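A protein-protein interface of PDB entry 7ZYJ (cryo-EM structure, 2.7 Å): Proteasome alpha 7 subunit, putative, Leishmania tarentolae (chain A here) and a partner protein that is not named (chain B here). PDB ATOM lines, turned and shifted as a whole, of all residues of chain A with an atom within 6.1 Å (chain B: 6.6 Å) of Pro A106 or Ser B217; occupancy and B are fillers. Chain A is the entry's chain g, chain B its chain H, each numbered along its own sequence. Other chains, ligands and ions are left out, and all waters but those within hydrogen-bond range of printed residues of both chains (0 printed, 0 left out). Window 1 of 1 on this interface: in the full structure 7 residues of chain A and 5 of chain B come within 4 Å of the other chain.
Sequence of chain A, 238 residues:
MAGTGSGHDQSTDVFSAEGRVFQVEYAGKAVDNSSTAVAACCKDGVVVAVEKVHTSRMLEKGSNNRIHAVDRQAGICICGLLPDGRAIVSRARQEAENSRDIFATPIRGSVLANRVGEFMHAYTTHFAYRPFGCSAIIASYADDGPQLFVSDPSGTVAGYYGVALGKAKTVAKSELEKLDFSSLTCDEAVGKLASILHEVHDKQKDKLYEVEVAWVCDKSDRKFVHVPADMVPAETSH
Printed residues of chain B within 4 Å of Pro A106: Ser B215, Ser B216 and Ser B217.
Ser B217 touches three residues of chain A.
Of the printed residues of chain B, Asp A143 touches Ser B217 (2.4 Å) and Ala B218 (3.0 Å).
Printed residues of chain B within 4 Å of Arg A72: Ser B215 and Ser B216.
Of the printed residues of chain B, Arg A100 touches Ser B215.
Of the printed residues of chain A, Ala B218 touches Thr A105 (3.7 Å) and Asp A143 (3.0 Å).
Of the printed residues of chain B, Thr A105 touches Ala B218.
Lys B219 touches none of the printed residues of chain A.
Asp A71 touches none of the printed residues of chain B.
The nearest residue of chain A that does not touch Ser B217 is Arg A100 (5.5 Å).
The nearest printed residue of chain A that does not touch Ser B215 is Gln A73 (4.6 Å).
Arg A72 touches Ser B215 (CD to C, 3.9 Å).
CB of Gln A73 touches OG of Ser B216 (3.3 Å).
OG1 of Thr A105 touches CB of Ala B218 (3.7 Å).
O of Ser B215 touches CG of Pro A106, 3.9 Å away.
CG of Pro A106 touches O of Ser B216, at 3.7 Å.
N of Ser B217 touches CG of Pro A106, at 3.9 Å.
NH2 of Arg A222 touches CB of Ser B217, at 3.7 Å.
The side-chain amide nitrogen (NE2) of Gln A73 sits at hydrogen-bond distance from the side-chain carboxylate (OD2) of Asp A71, at 3.4 Å.
OD1 of Asp A71 is in salt-bridge range of NE of Arg A100, 3.1 Å away.
O of Ser B217 is in hydrogen-bond range of OG of Ser B215 (2.7 Å).
The backbone NH (N) of Lys B219 sits close to the side-chain hydroxyl (OG) of Ser B217, at 3.4 Å.
The side-chain carboxylate of Asp A143 is in salt-bridge range of the guanidinium group of Arg A222, 3.9 Å away.
O of Thr A105 lies within hydrogen-bond range of OG of Ser A99.
Of the 7 printed residues of chain B, 4 touch a printed residue of chain A.
Hydrophobic or aromatic side chains of chain B that line the printed part of chain A: Ala B218.
Printed residues of chain A that touch a printed residue of chain B: Arg A72, Gln A73, Arg A100, Thr A105, Pro A106, Asp A143 and Arg A222.
Hydrophobic or aromatic side chains of chain A that line the printed part of chain B: Pro A106.
Among the printed residues, no Asp or Glu carboxylate lies within 4 Å of a Lys or Arg side-chain nitrogen of the other chain.
O of Ser B215 lies within hydrogen-bond range of NH1 of Arg A100 (3.0 Å).
OG of Ser B216 lies within hydrogen-bond range of NH1 of Arg A72, 2.8 Å away.
The side-chain hydroxyl of Ser B217 lies within hydrogen-bond range of the side-chain carboxylate of Asp A143 (2.4 Å).
The side-chain hydroxyl (OG) of Ser B216 is in hydrogen-bond range of the backbone carbonyl oxygen (O) of Arg A222 (2.6 Å).
The backbone NH of Ala B218 lies within hydrogen-bond range of the side-chain carboxylate of Asp A143, at 3.0 Å.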
ATOM      1  N   ASP A  71     -16.361 -24.825 -17.856  1.00  0.00           N
ATOM      2  CA  ASP A  71     -15.185 -25.255 -18.597  1.00  0.00           C
ATOM      3  C   ASP A  71     -15.234 -26.769 -18.736  1.00  0.00           C
ATOM      4  O   ASP A  71     -16.258 -27.385 -18.424  1.00  0.00           O
ATOM      5  CB  ASP A  71     -13.904 -24.804 -17.893  1.00  0.00           C
ATOM      6  CG  ASP A  71     -12.755 -24.586 -18.858  1.00  0.00           C
ATOM      7  OD1 ASP A  71     -12.867 -25.019 -20.023  1.00  0.00           O
ATOM      8  OD2 ASP A  71     -11.742 -23.980 -18.450  1.00  0.00           O
ATOM      9  N   ARG A  72     -14.149 -27.380 -19.213  1.00  0.00           N
ATOM     10  CA  ARG A  72     -14.114 -28.836 -19.286  1.00  0.00           C
ATOM     11  C   ARG A  72     -14.209 -29.453 -17.899  1.00  0.00           C
ATOM     12  O   ARG A  72     -14.902 -30.459 -17.702  1.00  0.00           O
ATOM     13  CB  ARG A  72     -12.842 -29.302 -19.991  1.00  0.00           C
ATOM     14  CG  ARG A  72     -12.804 -30.799 -20.244  1.00  0.00           C
ATOM     15  CD  ARG A  72     -11.529 -31.221 -20.951  1.00  0.00           C
ATOM     16  NE  ARG A  72     -11.559 -32.635 -21.306  1.00  0.00           N
ATOM     17  CZ  ARG A  72     -11.159 -33.617 -20.511  1.00  0.00           C
ATOM     18  NH1 ARG A  72     -10.684 -33.378 -19.300  1.00  0.00           N
ATOM     19  NH2 ARG A  72     -11.240 -34.873 -20.941  1.00  0.00           N
ATOM     20  N   GLN A  73     -13.533 -28.856 -16.921  1.00  0.00           N
ATOM     21  CA  GLN A  73     -13.455 -29.394 -15.571  1.00  0.00           C
ATOM     22  C   GLN A  73     -14.309 -28.636 -14.567  1.00  0.00           C
ATOM     23  O   GLN A  73     -14.344 -29.021 -13.394  1.00  0.00           O
ATOM     24  CB  GLN A  73     -11.998 -29.398 -15.096  1.00  0.00           C
ATOM     25  CG  GLN A  73     -11.464 -28.025 -14.718  1.00  0.00           C
ATOM     26  CD  GLN A  73     -11.168 -27.157 -15.924  1.00  0.00           C
ATOM     27  OE1 GLN A  73     -11.028 -27.653 -17.041  1.00  0.00           O
ATOM     28  NE2 GLN A  73     -11.075 -25.851 -15.706  1.00  0.00           N
ATOM     29  N   ALA A  96     -13.486 -18.423 -17.795  1.00  0.00           N
ATOM     30  CA  ALA A  96     -12.746 -19.661 -18.011  1.00  0.00           C
ATOM     31  C   ALA A  96     -12.019 -19.664 -19.348  1.00  0.00           C
ATOM     32  O   ALA A  96     -10.876 -20.128 -19.426  1.00  0.00           O
ATOM     33  CB  ALA A  96     -13.689 -20.859 -17.920  1.00  0.00           C
ATOM     34  N   SER A  99      -8.796 -17.422 -19.419  1.00  0.00           N
ATOM     35  CA  SER A  99      -7.608 -18.089 -18.900  1.00  0.00           C
ATOM     36  C   SER A  99      -7.007 -19.030 -19.937  1.00  0.00           C
ATOM     37  O   SER A  99      -5.782 -19.113 -20.077  1.00  0.00           O
ATOM     38  CB  SER A  99      -7.955 -18.849 -17.620  1.00  0.00           C
ATOM     39  OG  SER A  99      -6.815 -19.491 -17.079  1.00  0.00           O
ATOM     40  N   ARG A 100      -7.856 -19.746 -20.676  1.00  0.00           N
ATOM     41  CA  ARG A 100      -7.371 -20.693 -21.671  1.00  0.00           C
ATOM     42  C   ARG A 100      -6.821 -20.004 -22.912  1.00  0.00           C
ATOM     43  O   ARG A 100      -6.094 -20.638 -23.684  1.00  0.00           O
ATOM     44  CB  ARG A 100      -8.496 -21.650 -22.065  1.00  0.00           C
ATOM     45  CG  ARG A 100      -8.521 -22.937 -21.265  1.00  0.00           C
ATOM     46  CD  ARG A 100      -9.410 -23.970 -21.927  1.00  0.00           C
ATOM     47  NE  ARG A 100      -9.936 -24.930 -20.965  1.00  0.00           N
ATOM     48  CZ  ARG A 100      -9.279 -25.999 -20.537  1.00  0.00           C
ATOM     49  NH1 ARG A 100      -8.061 -26.278 -20.970  1.00  0.00           N
ATOM     50  NH2 ARG A 100      -9.858 -26.807 -19.655  1.00  0.00           N
ATOM     51  N   ALA A 104      -3.188 -19.730 -21.375  1.00  0.00           N
ATOM     52  CA  ALA A 104      -2.977 -21.086 -21.885  1.00  0.00           C
ATOM     53  C   ALA A 104      -2.981 -22.118 -20.760  1.00  0.00           C
ATOM     54  O   ALA A 104      -2.138 -23.017 -20.700  1.00  0.00           O
ATOM     55  CB  ALA A 104      -1.685 -21.167 -22.697  1.00  0.00           C
ATOM     56  N   THR A 105      -3.947 -21.982 -19.851  1.00  0.00           N
ATOM     57  CA  THR A 105      -4.077 -22.910 -18.743  1.00  0.00           C
ATOM     58  C   THR A 105      -5.530 -22.956 -18.296  1.00  0.00           C
ATOM     59  O   THR A 105      -6.224 -21.930 -18.363  1.00  0.00           O
ATOM     60  CB  THR A 105      -3.177 -22.522 -17.561  1.00  0.00           C
ATOM     61  OG1 THR A 105      -3.341 -23.466 -16.496  1.00  0.00           O
ATOM     62  CG2 THR A 105      -3.505 -21.125 -17.057  1.00  0.00           C
ATOM     63  N   PRO A 106      -6.028 -24.119 -17.878  1.00  0.00           N
ATOM     64  CA  PRO A 106      -7.372 -24.173 -17.295  1.00  0.00           C
ATOM     65  C   PRO A 106      -7.448 -23.323 -16.037  1.00  0.00           C
ATOM     66  O   PRO A 106      -6.489 -23.229 -15.269  1.00  0.00           O
ATOM     67  CB  PRO A 106      -7.566 -25.661 -16.984  1.00  0.00           C
ATOM     68  CG  PRO A 106      -6.620 -26.365 -17.894  1.00  0.00           C
ATOM     69  CD  PRO A 106      -5.437 -25.458 -18.034  1.00  0.00           C
ATOM     70  N   ILE A 107      -8.605 -22.696 -15.830  1.00  0.00           N
ATOM     71  CA  ILE A 107      -8.773 -21.810 -14.687  1.00  0.00           C
ATOM     72  C   ILE A 107      -8.904 -22.639 -13.416  1.00  0.00           C
ATOM     73  O   ILE A 107      -9.622 -23.646 -13.378  1.00  0.00           O
ATOM     74  CB  ILE A 107      -9.977 -20.876 -14.897  1.00  0.00           C
ATOM     75  CG1 ILE A 107     -10.009 -19.790 -13.819  1.00  0.00           C
ATOM     76  CG2 ILE A 107     -11.288 -21.653 -14.950  1.00  0.00           C
ATOM     77  CD1 ILE A 107     -10.976 -18.670 -14.117  1.00  0.00           C
ATOM     78  N   ARG A 108      -8.172 -22.241 -12.379  1.00  0.00           N
ATOM     79  CA  ARG A 108      -8.253 -22.923 -11.098  1.00  0.00           C
ATOM     80  C   ARG A 108      -9.621 -22.695 -10.466  1.00  0.00           C
ATOM     81  O   ARG A 108     -10.266 -21.665 -10.683  1.00  0.00           O
ATOM     82  CB  ARG A 108      -7.147 -22.431 -10.165  1.00  0.00           C
ATOM     83  CG  ARG A 108      -5.744 -22.693 -10.693  1.00  0.00           C
ATOM     84  CD  ARG A 108      -4.687 -21.960  -9.884  1.00  0.00           C
ATOM     85  NE  ARG A 108      -4.448 -22.570  -8.582  1.00  0.00           N
ATOM     86  CZ  ARG A 108      -3.533 -23.501  -8.350  1.00  0.00           C
ATOM     87  NH1 ARG A 108      -2.757 -23.965  -9.316  1.00  0.00           N
ATOM     88  NH2 ARG A 108      -3.388 -23.976  -7.117  1.00  0.00           N
ATOM     89  N   ALA A 142      -9.617 -28.875 -10.994  1.00  0.00           N
ATOM     90  CA  ALA A 142      -8.503 -28.242 -11.674  1.00  0.00           C
ATOM     91  C   ALA A 142      -7.186 -28.743 -11.084  1.00  0.00           C
ATOM     92  O   ALA A 142      -7.149 -29.712 -10.319  1.00  0.00           O
ATOM     93  CB  ALA A 142      -8.633 -26.720 -11.596  1.00  0.00           C
ATOM     94  N   ASP A 143      -6.088 -28.083 -11.450  1.00  0.00           N
ATOM     95  CA  ASP A 143      -4.762 -28.476 -10.987  1.00  0.00           C
ATOM     96  C   ASP A 143      -4.606 -28.292  -9.483  1.00  0.00           C
ATOM     97  O   ASP A 143      -3.649 -28.800  -8.890  1.00  0.00           O
ATOM     98  CB  ASP A 143      -3.686 -27.681 -11.729  1.00  0.00           C
ATOM     99  CG  ASP A 143      -3.334 -28.289 -13.070  1.00  0.00           C
ATOM    100  OD1 ASP A 143      -3.378 -29.531 -13.189  1.00  0.00           O
ATOM    101  OD2 ASP A 143      -3.016 -27.527 -14.006  1.00  0.00           O
ATOM    102  N   ARG A 222     -11.853 -36.280 -15.495  1.00  0.00           N
ATOM    103  CA  ARG A 222     -11.837 -34.939 -14.909  1.00  0.00           C
ATOM    104  C   ARG A 222     -12.621 -33.945 -15.763  1.00  0.00           C
ATOM    105  O   ARG A 222     -12.239 -32.784 -15.906  1.00  0.00           O
ATOM    106  CB  ARG A 222     -10.403 -34.456 -14.685  1.00  0.00           C
ATOM    107  CG  ARG A 222      -9.663 -35.237 -13.616  1.00  0.00           C
ATOM    108  CD  ARG A 222      -8.173 -34.950 -13.646  1.00  0.00           C
ATOM    109  NE  ARG A 222      -7.896 -33.521 -13.577  1.00  0.00           N
ATOM    110  CZ  ARG A 222      -6.727 -33.001 -13.229  1.00  0.00           C
ATOM    111  NH1 ARG A 222      -5.699 -33.767 -12.905  1.00  0.00           N
ATOM    112  NH2 ARG A 222      -6.586 -31.679 -13.203  1.00  0.00           N
ATOM    113  N   PRO B 213      -4.085 -31.990 -26.821  1.00  0.00           N
ATOM    114  CA  PRO B 213      -5.476 -32.406 -26.628  1.00  0.00           C
ATOM    115  C   PRO B 213      -6.154 -31.511 -25.605  1.00  0.00           C
ATOM    116  O   PRO B 213      -5.514 -30.967 -24.702  1.00  0.00           O
ATOM    117  CB  PRO B 213      -5.355 -33.846 -26.116  1.00  0.00           C
ATOM    118  CG  PRO B 213      -3.964 -34.275 -26.456  1.00  0.00           C
ATOM    119  CD  PRO B 213      -3.132 -33.032 -26.410  1.00  0.00           C
ATOM    120  N   SER B 215      -7.668 -30.682 -22.432  1.00  0.00           N
ATOM    121  CA  SER B 215      -7.448 -31.342 -21.155  1.00  0.00           C
ATOM    122  C   SER B 215      -7.866 -30.432 -20.010  1.00  0.00           C
ATOM    123  O   SER B 215      -7.951 -29.210 -20.152  1.00  0.00           O
ATOM    124  CB  SER B 215      -5.979 -31.754 -20.981  1.00  0.00           C
ATOM    125  OG  SER B 215      -5.184 -30.645 -20.599  1.00  0.00           O
ATOM    126  N   SER B 216      -8.126 -31.056 -18.864  1.00  0.00           N
ATOM    127  CA  SER B 216      -8.489 -30.344 -17.649  1.00  0.00           C
ATOM    128  C   SER B 216      -7.281 -29.910 -16.832  1.00  0.00           C
ATOM    129  O   SER B 216      -7.457 -29.295 -15.774  1.00  0.00           O
ATOM    130  CB  SER B 216      -9.399 -31.219 -16.782  1.00  0.00           C
ATOM    131  OG  SER B 216     -10.686 -31.346 -17.360  1.00  0.00           O
ATOM    132  N   SER B 217      -6.071 -30.210 -17.290  1.00  0.00           N
ATOM    133  CA  SER B 217      -4.847 -29.908 -16.566  1.00  0.00           C
ATOM    134  C   SER B 217      -3.877 -29.155 -17.466  1.00  0.00           C
ATOM    135  O   SER B 217      -3.975 -29.186 -18.696  1.00  0.00           O
ATOM    136  CB  SER B 217      -4.188 -31.190 -16.041  1.00  0.00           C
ATOM    137  OG  SER B 217      -3.122 -30.890 -15.158  1.00  0.00           O
ATOM    138  N   ALA B 218      -2.930 -28.471 -16.831  1.00  0.00           N
ATOM    139  CA  ALA B 218      -1.858 -27.778 -17.532  1.00  0.00           C
ATOM    140  C   ALA B 218      -0.691 -28.695 -17.871  1.00  0.00           C
ATOM    141  O   ALA B 218       0.277 -28.241 -18.486  1.00  0.00           O
ATOM    142  CB  ALA B 218      -1.360 -26.595 -16.698  1.00  0.00           C
ATOM    143  N   LYS B 219      -0.762 -29.965 -17.482  1.00  0.00           N
ATOM    144  CA  LYS B 219       0.300 -30.914 -17.790  1.00  0.00           C
ATOM    145  C   LYS B 219       0.347 -31.195 -19.286  1.00  0.00           C
ATOM    146  O   LYS B 219      -0.675 -31.506 -19.905  1.00  0.00           O
ATOM    147  CB  LYS B 219       0.083 -32.212 -17.015  1.00  0.00           C
ATOM    148  CG  LYS B 219       1.136 -33.281 -17.259  1.00  0.00           C
ATOM    149  CD  LYS B 219       2.490 -32.874 -16.705  1.00  0.00           C
ATOM    150  CE  LYS B 219       3.491 -34.013 -16.816  1.00  0.00           C
ATOM    151  NZ  LYS B 219       3.812 -34.340 -18.233  1.00  0.00           N
ATOM    152  N   ILE B 220       1.538 -31.091 -19.867  1.00  0.00           N
ATOM    153  CA  ILE B 220       1.726 -31.371 -21.284  1.00  0.00           C
ATOM    154  C   ILE B 220       1.958 -32.865 -21.461  1.00  0.00           C
ATOM    155  O   ILE B 220       2.869 -33.441 -20.856  1.00  0.00           O
ATOM    156  CB  ILE B 220       2.897 -30.552 -21.847  1.00  0.00           C
ATOM    157  CG1 ILE B 220       2.552 -29.062 -21.839  1.00  0.00           C
ATOM    158  CG2 ILE B 220       3.238 -31.007 -23.250  1.00  0.00           C
ATOM    159  CD1 ILE B 220       3.752 -28.157 -21.965  1.00  0.00           C
